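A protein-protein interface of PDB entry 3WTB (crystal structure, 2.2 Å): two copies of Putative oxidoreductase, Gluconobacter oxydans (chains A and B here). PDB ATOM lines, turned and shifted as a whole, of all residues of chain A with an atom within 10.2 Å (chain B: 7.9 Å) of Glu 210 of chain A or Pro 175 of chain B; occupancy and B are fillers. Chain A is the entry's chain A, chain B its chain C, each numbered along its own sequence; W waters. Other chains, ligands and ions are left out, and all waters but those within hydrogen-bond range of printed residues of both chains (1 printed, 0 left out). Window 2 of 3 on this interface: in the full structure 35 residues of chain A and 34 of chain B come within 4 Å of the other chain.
The backbone NH of Gly 242 of chain A sits at hydrogen-bond distance from the backbone carbonyl oxygen of Tyr 232 of chain B (2.9 Å).
The backbone carbonyl oxygen of Phe 206 of chain A lies within hydrogen-bond range of the guanidinium group of Arg 171 of chain B (2.9 Å).
OH of Tyr 232 of chain B lies within hydrogen-bond range of O of Pro 187 of chain A (3.1 Å).
The side-chain hydroxyl of Tyr 232 of chain B sits close to the backbone NH of Gly 213 of chain A (3.2 Å).
N of Asp 241 of chain A sits at hydrogen-bond distance from O of Tyr 232 of chain B (3.4 Å).
The backbone carbonyl oxygen (O) of Ser 211 of chain A lies within hydrogen-bond range of the side-chain hydroxyl (OH) of Tyr 232 of chain B.
The backbone carbonyl oxygen (O) of Leu 244 of chain A is in hydrogen-bond range of the guanidinium group (NH2) of Arg 171 of chain B (3.1 Å).
The backbone carbonyl oxygen of Gly 243 of chain A lies within hydrogen-bond range of the guanidinium group of Arg 171 of chain B (3.2 Å).
OG1 of Thr 207 of chain A lies within hydrogen-bond range of N of Glu 210 of chain A, at 2.8 Å.
The backbone NH (N) of Ala 208 of chain A sits at hydrogen-bond distance from the backbone carbonyl oxygen (O) of Gly 242 of chain A (2.8 Å).
The backbone NH of Thr 209 of chain A lies within hydrogen-bond range of the backbone carbonyl oxygen of Gly 242 of chain A, 3.0 Å away.
The backbone carbonyl oxygen of Pro 187 of chain A is in hydrogen-bond range of the backbone NH of Gly 213 of chain A (2.9 Å).
OD1 of Asp 241 of chain A sits at hydrogen-bond distance from N of Gly 243 of chain A, at 2.9 Å.
OD2 of Asp 241 of chain A lies within hydrogen-bond range of N of Leu 244 of chain A.
Among the printed residues, merely in contact across the chains: Ala 208 of chain A with Gly 174 of chain B (3.3 Å), Ala 208 of chain A with Pro 175 of chain B (3.4 Å), Tyr 212 of chain A with Tyr 232 of chain B (3.5 Å), Ala 208 of chain A with Ala 170 of chain B (3.5 Å), Ala 208 of chain A with Arg 171 of chain B (3.6 Å), Thr 207 of chain A with Arg 171 of chain B (3.7 Å), Thr 209 of chain A with Tyr 232 of chain B (3.7 Å), Glu 210 of chain A with Pro 175 of chain B (3.8 Å), Thr 209 of chain A with Gly 174 of chain B (3.9 Å) and Thr 207 of chain A with Tyr 232 of chain B (3.9 Å).
Of the printed residues of chain B, Glu 210 of chain A touches Pro 175 (3.8 Å).
Of chain A, only Ala 208 and Glu 210 come within 4 Å of Pro 175 of chain B.
Gly 174 of chain B touches just these residues of chain A: Ala 208 (3.3 Å) and Thr 209 (3.9 Å).
Of the printed residues of chain B, Thr 209 of chain A touches Gly 174 and Tyr 232.
Of the printed residues of chain B, Thr 207 of chain A touches Arg 171 and Tyr 232.
Asp 196 of chain A touches none of the printed residues of chain B.
Ala 201 of chain A touches none of the printed residues of chain B.
Hydrophobic or aromatic side chains of chain A that line the printed part of chain B: Pro 187 and Ala 208.
Along chain A the printed residues that touch a printed residue of chain B span positions 187 to 244.
Hydrophobic or aromatic side chains of chain B within 4 Å of the printed part of chain A: Pro 175 and Tyr 232.
Among the printed residues, no Asp or Glu carboxylate lies within 4 Å of a Lys or Arg side-chain nitrogen of the other chain.
No position is printed for both chains.
Of the 18 pairs that touch across the chains among the printed residues, none has its exchanged pair printed and touching as well.
Water W1 bridges the guanidinium group (NH1) of Arg 171 of chain B (2.6 Å) and the backbone carbonyl oxygen (O) of Thr 207 of chain A (3.0 Å).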
ATOM      1  N   PRO A 187      20.796  26.536  -0.579  1.00  0.00           N
ATOM      2  CA  PRO A 187      20.448  27.946  -0.492  1.00  0.00           C
ATOM      3  C   PRO A 187      20.057  28.456  -1.877  1.00  0.00           C
ATOM      4  O   PRO A 187      20.855  28.363  -2.846  1.00  0.00           O
ATOM      5  CB  PRO A 187      21.768  28.612  -0.032  1.00  0.00           C
ATOM      6  CG  PRO A 187      22.850  27.698  -0.538  1.00  0.00           C
ATOM      7  CD  PRO A 187      22.253  26.312  -0.616  1.00  0.00           C
ATOM      8  N   GLU A 195      21.419  36.497  -2.052  1.00  0.00           N
ATOM      9  CA  GLU A 195      22.765  35.877  -2.252  1.00  0.00           C
ATOM     10  C   GLU A 195      23.972  36.720  -1.827  1.00  0.00           C
ATOM     11  O   GLU A 195      25.083  36.193  -1.808  1.00  0.00           O
ATOM     12  CB  GLU A 195      23.086  35.466  -3.731  1.00  0.00           C
ATOM     13  CG  GLU A 195      22.215  35.949  -4.869  1.00  0.00           C
ATOM     14  CD  GLU A 195      22.864  35.445  -6.131  1.00  0.00           C
ATOM     15  OE1 GLU A 195      23.593  36.211  -6.736  1.00  0.00           O
ATOM     16  OE2 GLU A 195      22.761  34.253  -6.454  1.00  0.00           O
ATOM     17  N   ASP A 196      23.772  37.998  -1.523  1.00  0.00           N
ATOM     18  CA  ASP A 196      24.886  38.922  -1.150  1.00  0.00           C
ATOM     19  C   ASP A 196      24.864  39.099   0.380  1.00  0.00           C
ATOM     20  O   ASP A 196      23.863  38.790   1.074  1.00  0.00           O
ATOM     21  CB  ASP A 196      24.960  40.282  -1.958  1.00  0.00           C
ATOM     22  CG  ASP A 196      23.627  41.043  -1.985  1.00  0.00           C
ATOM     23  OD1 ASP A 196      22.597  40.404  -2.229  1.00  0.00           O
ATOM     24  OD2 ASP A 196      23.626  42.284  -1.800  1.00  0.00           O
ATOM     25  N   ALA A 200      25.330  35.133   3.860  1.00  0.00           N
ATOM     26  CA  ALA A 200      25.269  34.342   2.656  1.00  0.00           C
ATOM     27  C   ALA A 200      26.661  33.846   2.226  1.00  0.00           C
ATOM     28  O   ALA A 200      26.759  32.701   1.793  1.00  0.00           O
ATOM     29  CB  ALA A 200      24.645  35.152   1.533  1.00  0.00           C
ATOM     30  N   ALA A 201      27.704  34.668   2.396  1.00  0.00           N
ATOM     31  CA  ALA A 201      29.094  34.240   2.120  1.00  0.00           C
ATOM     32  C   ALA A 201      29.524  33.032   2.990  1.00  0.00           C
ATOM     33  O   ALA A 201      30.165  32.100   2.503  1.00  0.00           O
ATOM     34  CB  ALA A 201      30.073  35.350   2.302  1.00  0.00           C
ATOM     35  N   VAL A 202      29.043  32.971   4.230  1.00  0.00           N
ATOM     36  CA  VAL A 202      29.309  31.815   5.069  1.00  0.00           C
ATOM     37  C   VAL A 202      28.598  30.569   4.549  1.00  0.00           C
ATOM     38  O   VAL A 202      29.238  29.510   4.385  1.00  0.00           O
ATOM     39  CB  VAL A 202      28.966  32.086   6.551  1.00  0.00           C
ATOM     40  CG1 VAL A 202      29.016  30.800   7.385  1.00  0.00           C
ATOM     41  CG2 VAL A 202      29.928  33.136   7.102  1.00  0.00           C
ATOM     42  N   ILE A 203      27.292  30.661   4.303  1.00  0.00           N
ATOM     43  CA  ILE A 203      26.533  29.498   3.789  1.00  0.00           C
ATOM     44  C   ILE A 203      27.103  29.020   2.476  1.00  0.00           C
ATOM     45  O   ILE A 203      27.273  27.829   2.225  1.00  0.00           O
ATOM     46  CB  ILE A 203      25.045  29.816   3.600  1.00  0.00           C
ATOM     47  CG1 ILE A 203      24.431  30.137   4.966  1.00  0.00           C
ATOM     48  CG2 ILE A 203      24.282  28.651   2.922  1.00  0.00           C
ATOM     49  CD1 ILE A 203      22.923  30.366   4.936  1.00  0.00           C
ATOM     50  N   ARG A 204      27.421  29.956   1.632  1.00  0.00           N
ATOM     51  CA  ARG A 204      27.923  29.679   0.295  1.00  0.00           C
ATOM     52  C   ARG A 204      29.211  28.834   0.320  1.00  0.00           C
ATOM     53  O   ARG A 204      29.431  28.021  -0.557  1.00  0.00           O
ATOM     54  CB  ARG A 204      28.182  31.026  -0.367  1.00  0.00           C
ATOM     55  CG  ARG A 204      28.629  31.031  -1.770  1.00  0.00           C
ATOM     56  CD  ARG A 204      29.047  32.420  -2.206  1.00  0.00           C
ATOM     57  NE  ARG A 204      27.890  33.259  -2.395  1.00  0.00           N
ATOM     58  CZ  ARG A 204      27.936  34.498  -2.845  1.00  0.00           C
ATOM     59  NH1 ARG A 204      29.114  35.081  -3.039  1.00  0.00           N
ATOM     60  NH2 ARG A 204      26.809  35.157  -3.077  1.00  0.00           N
ATOM     61  N   LYS A 205      30.079  29.088   1.302  1.00  0.00           N
ATOM     62  CA  LYS A 205      31.314  28.335   1.443  1.00  0.00           C
ATOM     63  C   LYS A 205      31.103  26.860   1.709  1.00  0.00           C
ATOM     64  O   LYS A 205      32.000  26.107   1.489  1.00  0.00           O
ATOM     65  CB  LYS A 205      32.201  28.917   2.555  1.00  0.00           C
ATOM     66  CG  LYS A 205      32.926  30.181   2.097  1.00  0.00           C
ATOM     67  CD  LYS A 205      34.045  30.577   3.048  1.00  0.00           C
ATOM     68  CE  LYS A 205      34.630  31.931   2.662  1.00  0.00           C
ATOM     69  NZ  LYS A 205      35.420  32.485   3.791  1.00  0.00           N
ATOM     70  N   PHE A 206      29.935  26.463   2.205  1.00  0.00           N
ATOM     71  CA  PHE A 206      29.637  25.053   2.359  1.00  0.00           C
ATOM     72  C   PHE A 206      29.204  24.366   1.023  1.00  0.00           C
ATOM     73  O   PHE A 206      29.217  23.149   0.953  1.00  0.00           O
ATOM     74  CB  PHE A 206      28.579  24.808   3.447  1.00  0.00           C
ATOM     75  CG  PHE A 206      29.103  25.051   4.824  1.00  0.00           C
ATOM     76  CD1 PHE A 206      30.007  24.182   5.365  1.00  0.00           C
ATOM     77  CD2 PHE A 206      28.711  26.175   5.562  1.00  0.00           C
ATOM     78  CE1 PHE A 206      30.517  24.415   6.655  1.00  0.00           C
ATOM     79  CE2 PHE A 206      29.213  26.412   6.842  1.00  0.00           C
ATOM     80  CZ  PHE A 206      30.124  25.522   7.391  1.00  0.00           C
ATOM     81  N   THR A 207      28.808  25.147   0.032  1.00  0.00           N
ATOM     82  CA  THR A 207      28.486  24.611  -1.249  1.00  0.00           C
ATOM     83  C   THR A 207      29.768  24.350  -2.015  1.00  0.00           C
ATOM     84  O   THR A 207      30.742  25.034  -1.830  1.00  0.00           O
ATOM     85  CB  THR A 207      27.605  25.556  -2.110  1.00  0.00           C
ATOM     86  OG1 THR A 207      28.318  26.713  -2.441  1.00  0.00           O
ATOM     87  CG2 THR A 207      26.336  25.913  -1.451  1.00  0.00           C
ATOM     88  N   ALA A 208      29.754  23.378  -2.903  1.00  0.00           N
ATOM     89  CA  ALA A 208      30.931  23.125  -3.723  1.00  0.00           C
ATOM     90  C   ALA A 208      31.064  24.192  -4.801  1.00  0.00           C
ATOM     91  O   ALA A 208      32.166  24.540  -5.191  1.00  0.00           O
ATOM     92  CB  ALA A 208      30.857  21.730  -4.351  1.00  0.00           C
ATOM     93  N   THR A 209      29.943  24.703  -5.320  1.00  0.00           N
ATOM     94  CA  THR A 209      29.981  25.704  -6.364  1.00  0.00           C
ATOM     95  C   THR A 209      30.250  27.106  -5.794  1.00  0.00           C
ATOM     96  O   THR A 209      30.490  27.997  -6.558  1.00  0.00           O
ATOM     97  CB  THR A 209      28.654  25.807  -7.102  1.00  0.00           C
ATOM     98  OG1 THR A 209      27.620  26.119  -6.160  1.00  0.00           O
ATOM     99  CG2 THR A 209      28.327  24.499  -7.830  1.00  0.00           C
ATOM    100  N   GLU A 210      30.202  27.266  -4.465  1.00  0.00           N
ATOM    101  CA  GLU A 210      30.429  28.556  -3.808  1.00  0.00           C
ATOM    102  C   GLU A 210      29.428  29.589  -4.290  1.00  0.00           C
ATOM    103  O   GLU A 210      29.789  30.698  -4.630  1.00  0.00           O
ATOM    104  CB  GLU A 210      31.908  29.029  -4.009  1.00  0.00           C
ATOM    105  CG  GLU A 210      32.876  27.992  -3.448  1.00  0.00           C
ATOM    106  CD  GLU A 210      34.356  28.170  -3.821  1.00  0.00           C
ATOM    107  OE1 GLU A 210      34.702  29.018  -4.677  1.00  0.00           O
ATOM    108  OE2 GLU A 210      35.193  27.451  -3.223  1.00  0.00           O
ATOM    109  N   SER A 211      28.182  29.154  -4.392  1.00  0.00           N
ATOM    110  CA  SER A 211      27.122  29.966  -4.913  1.00  0.00           C
ATOM    111  C   SER A 211      25.794  29.552  -4.354  1.00  0.00           C
ATOM    112  O   SER A 211      25.583  28.393  -3.951  1.00  0.00           O
ATOM    113  CB  SER A 211      27.104  29.887  -6.464  1.00  0.00           C
ATOM    114  OG  SER A 211      26.752  28.582  -6.915  1.00  0.00           O
ATOM    115  N   TYR A 212      24.860  30.491  -4.395  1.00  0.00           N
ATOM    116  CA  TYR A 212      23.445  30.221  -4.204  1.00  0.00           C
ATOM    117  C   TYR A 212      22.849  29.830  -5.515  1.00  0.00           C
ATOM    118  O   TYR A 212      23.328  30.258  -6.558  1.00  0.00           O
ATOM    119  CB  TYR A 212      22.704  31.481  -3.751  1.00  0.00           C
ATOM    120  CG  TYR A 212      22.683  31.693  -2.255  1.00  0.00           C
ATOM    121  CD1 TYR A 212      23.806  31.429  -1.474  1.00  0.00           C
ATOM    122  CD2 TYR A 212      21.544  32.161  -1.627  1.00  0.00           C
ATOM    123  CE1 TYR A 212      23.782  31.628  -0.103  1.00  0.00           C
ATOM    124  CE2 TYR A 212      21.508  32.373  -0.248  1.00  0.00           C
ATOM    125  CZ  TYR A 212      22.633  32.121   0.505  1.00  0.00           C
ATOM    126  OH  TYR A 212      22.623  32.342   1.843  1.00  0.00           O
ATOM    127  N   GLY A 213      21.782  29.026  -5.466  1.00  0.00           N
ATOM    128  CA  GLY A 213      21.009  28.694  -6.657  1.00  0.00           C
ATOM    129  C   GLY A 213      19.907  29.715  -6.930  1.00  0.00           C
ATOM    130  O   GLY A 213      19.838  30.741  -6.261  1.00  0.00           O
ATOM    131  N   ASP A 241      21.614  21.573  -4.692  1.00  0.00           N
ATOM    132  CA  ASP A 241      22.278  22.267  -3.595  1.00  0.00           C
ATOM    133  C   ASP A 241      23.690  22.742  -3.844  1.00  0.00           C
ATOM    134  O   ASP A 241      24.404  23.064  -2.914  1.00  0.00           O
ATOM    135  CB  ASP A 241      22.271  21.377  -2.384  1.00  0.00           C
ATOM    136  CG  ASP A 241      23.292  20.217  -2.493  1.00  0.00           C
ATOM    137  OD1 ASP A 241      23.737  19.853  -3.634  1.00  0.00           O
ATOM    138  OD2 ASP A 241      23.607  19.647  -1.421  1.00  0.00           O
ATOM    139  N   GLY A 242      24.116  22.776  -5.085  1.00  0.00           N
ATOM    140  CA  GLY A 242      25.438  23.235  -5.406  1.00  0.00           C
ATOM    141  C   GLY A 242      26.504  22.441  -4.738  1.00  0.00           C
ATOM    142  O   GLY A 242      27.628  22.935  -4.608  1.00  0.00           O
ATOM    143  N   GLY A 243      26.205  21.198  -4.361  1.00  0.00           N
ATOM    144  CA  GLY A 243      27.233  20.360  -3.760  1.00  0.00           C
ATOM    145  C   GLY A 243      27.382  20.521  -2.256  1.00  0.00           C
ATOM    146  O   GLY A 243      28.345  20.039  -1.669  1.00  0.00           O
ATOM    147  N   LEU A 244      26.401  21.140  -1.609  1.00  0.00           N
ATOM    148  CA  LEU A 244      26.500  21.377  -0.190  1.00  0.00           C
ATOM    149  C   LEU A 244      26.638  20.073   0.574  1.00  0.00           C
ATOM    150  O   LEU A 244      27.490  19.948   1.440  1.00  0.00           O
ATOM    151  CB  LEU A 244      25.290  22.180   0.318  1.00  0.00           C
ATOM    152  CG  LEU A 244      25.430  22.545   1.778  1.00  0.00           C
ATOM    153  CD1 LEU A 244      25.065  24.005   2.016  1.00  0.00           C
ATOM    154  CD2 LEU A 244      24.563  21.609   2.581  1.00  0.00           C
ATOM    155  N   THR B 132      34.507  24.434 -18.052  1.00  0.00           N
ATOM    156  CA  THR B 132      33.339  24.926 -17.345  1.00  0.00           C
ATOM    157  C   THR B 132      32.086  24.598 -18.179  1.00  0.00           C
ATOM    158  O   THR B 132      32.087  24.751 -19.392  1.00  0.00           O
ATOM    159  CB  THR B 132      33.455  26.428 -16.973  1.00  0.00           C
ATOM    160  OG1 THR B 132      32.257  26.839 -16.323  1.00  0.00           O
ATOM    161  CG2 THR B 132      33.621  27.322 -18.192  1.00  0.00           C
ATOM    162  N   VAL B 169      34.380  14.145  -6.159  1.00  0.00           N
ATOM    163  CA  VAL B 169      34.629  14.812  -7.416  1.00  0.00           C
ATOM    164  C   VAL B 169      33.819  16.066  -7.529  1.00  0.00           C
ATOM    165  O   VAL B 169      34.332  17.088  -7.948  1.00  0.00           O
ATOM    166  CB  VAL B 169      34.356  13.877  -8.612  1.00  0.00           C
ATOM    167  CG1 VAL B 169      34.381  14.613  -9.949  1.00  0.00           C
ATOM    168  CG2 VAL B 169      35.389  12.790  -8.626  1.00  0.00           C
ATOM    169  N   ALA B 170      32.569  16.024  -7.092  1.00  0.00           N
ATOM    170  CA  ALA B 170      31.720  17.217  -7.079  1.00  0.00           C
ATOM    171  C   ALA B 170      32.344  18.300  -6.237  1.00  0.00           C
ATOM    172  O   ALA B 170      32.354  19.466  -6.617  1.00  0.00           O
ATOM    173  CB  ALA B 170      30.317  16.874  -6.568  1.00  0.00           C
ATOM    174  N   ARG B 171      32.827  17.906  -5.075  1.00  0.00           N
ATOM    175  CA  ARG B 171      33.486  18.829  -4.208  1.00  0.00           C
ATOM    176  C   ARG B 171      34.720  19.449  -4.884  1.00  0.00           C
ATOM    177  O   ARG B 171      34.904  20.660  -4.844  1.00  0.00           O
ATOM    178  CB  ARG B 171      33.833  18.125  -2.908  1.00  0.00           C
ATOM    179  CG  ARG B 171      34.484  19.018  -1.857  1.00  0.00           C
ATOM    180  CD  ARG B 171      33.562  20.067  -1.244  1.00  0.00           C
ATOM    181  NE  ARG B 171      32.435  19.497  -0.505  1.00  0.00           N
ATOM    182  CZ  ARG B 171      31.388  20.205  -0.054  1.00  0.00           C
ATOM    183  NH1 ARG B 171      31.309  21.505  -0.310  1.00  0.00           N
ATOM    184  NH2 ARG B 171      30.449  19.635   0.704  1.00  0.00           N
ATOM    185  N   ASP B 172      35.554  18.627  -5.509  1.00  0.00           N
ATOM    186  CA  ASP B 172      36.752  19.124  -6.185  1.00  0.00           C
ATOM    187  C   ASP B 172      36.438  20.064  -7.322  1.00  0.00           C
ATOM    188  O   ASP B 172      37.209  21.009  -7.563  1.00  0.00           O
ATOM    189  CB  ASP B 172      37.569  17.974  -6.846  1.00  0.00           C
ATOM    190  CG  ASP B 172      38.383  17.156  -5.871  1.00  0.00           C
ATOM    191  OD1 ASP B 172      38.160  17.259  -4.635  1.00  0.00           O
ATOM    192  OD2 ASP B 172      39.212  16.296  -6.345  1.00  0.00           O
ATOM    193  N   LEU B 173      35.405  19.751  -8.117  1.00  0.00           N
ATOM    194  CA  LEU B 173      35.189  20.457  -9.369  1.00  0.00           C
ATOM    195  C   LEU B 173      34.188  21.600  -9.293  1.00  0.00           C
ATOM    196  O   LEU B 173      33.975  22.329 -10.273  1.00  0.00           O
ATOM    197  CB  LEU B 173      34.754  19.491 -10.453  1.00  0.00           C
ATOM    198  CG  LEU B 173      35.759  18.361 -10.694  1.00  0.00           C
ATOM    199  CD1 LEU B 173      35.266  17.488 -11.803  1.00  0.00           C
ATOM    200  CD2 LEU B 173      37.149  18.865 -11.026  1.00  0.00           C
ATOM    201  N   GLY B 174      33.571  21.756  -8.137  1.00  0.00           N
ATOM    202  CA  GLY B 174      32.591  22.799  -7.943  1.00  0.00           C
ATOM    203  C   GLY B 174      33.023  24.111  -8.522  1.00  0.00           C
ATOM    204  O   GLY B 174      32.280  24.681  -9.314  1.00  0.00           O
ATOM    205  N   PRO B 175      34.209  24.623  -8.107  1.00  0.00           N
ATOM    206  CA  PRO B 175      34.541  25.997  -8.503  1.00  0.00           C
ATOM    207  C   PRO B 175      34.962  26.069  -9.981  1.00  0.00           C
ATOM    208  O   PRO B 175      35.020  27.159 -10.526  1.00  0.00           O
ATOM    209  CB  PRO B 175      35.719  26.386  -7.595  1.00  0.00           C
ATOM    210  CG  PRO B 175      35.667  25.429  -6.449  1.00  0.00           C
ATOM    211  CD  PRO B 175      35.030  24.162  -6.983  1.00  0.00           C
ATOM    212  N   GLN B 176      35.157  24.927 -10.620  1.00  0.00           N
ATOM    213  CA  GLN B 176      35.485  24.905 -12.035  1.00  0.00           C
ATOM    214  C   GLN B 176      34.268  24.819 -12.948  1.00  0.00           C
ATOM    215  O   GLN B 176      34.412  24.859 -14.150  1.00  0.00           O
ATOM    216  CB  GLN B 176      36.388  23.720 -12.314  1.00  0.00           C
ATOM    217  CG  GLN B 176      37.718  23.855 -11.611  1.00  0.00           C
ATOM    218  CD  GLN B 176      38.529  22.545 -11.687  1.00  0.00           C
ATOM    219  OE1 GLN B 176      38.658  21.926 -12.743  1.00  0.00           O
ATOM    220  NE2 GLN B 176      39.064  22.150 -10.570  1.00  0.00           N
ATOM    221  N   GLY B 177      33.063  24.718 -12.386  1.00  0.00           N
ATOM    222  CA  GLY B 177      31.856  24.714 -13.181  1.00  0.00           C
ATOM    223  C   GLY B 177      31.625  23.389 -13.924  1.00  0.00           C
ATOM    224  O   GLY B 177      30.907  23.354 -14.902  1.00  0.00           O
ATOM    225  N   ILE B 178      32.188  22.309 -13.411  1.00  0.00           N
ATOM    226  CA  ILE B 178      31.861  20.977 -13.891  1.00  0.00           C
ATOM    227  C   ILE B 178      31.062  20.284 -12.790  1.00  0.00           C
ATOM    228  O   ILE B 178      31.428  20.358 -11.599  1.00  0.00           O
ATOM    229  CB  ILE B 178      33.142  20.206 -14.195  1.00  0.00           C
ATOM    230  CG1 ILE B 178      33.929  20.931 -15.326  1.00  0.00           C
ATOM    231  CG2 ILE B 178      32.853  18.788 -14.579  1.00  0.00           C
ATOM    232  CD1 ILE B 178      35.334  20.401 -15.543  1.00  0.00           C
ATOM    233  N   TYR B 232      23.271  23.690 -11.000  1.00  0.00           N
ATOM    234  CA  TYR B 232      23.242  23.685  -9.535  1.00  0.00           C
ATOM    235  C   TYR B 232      23.079  22.285  -8.964  1.00  0.00           C
ATOM    236  O   TYR B 232      23.040  22.122  -7.745  1.00  0.00           O
ATOM    237  CB  TYR B 232      22.178  24.615  -8.979  1.00  0.00           C
ATOM    238  CG  TYR B 232      22.495  25.159  -7.615  1.00  0.00           C
ATOM    239  CD1 TYR B 232      23.640  25.911  -7.399  1.00  0.00           C
ATOM    240  CD2 TYR B 232      21.621  24.956  -6.521  1.00  0.00           C
ATOM    241  CE1 TYR B 232      23.914  26.400  -6.150  1.00  0.00           C
ATOM    242  CE2 TYR B 232      21.900  25.433  -5.292  1.00  0.00           C
ATOM    243  CZ  TYR B 232      23.051  26.152  -5.096  1.00  0.00           C
ATOM    244  OH  TYR B 232      23.320  26.720  -3.860  1.00  0.00           O
HETATM  245  O   HOH W   1      33.033  23.434  -0.716  1.00  0.00           O
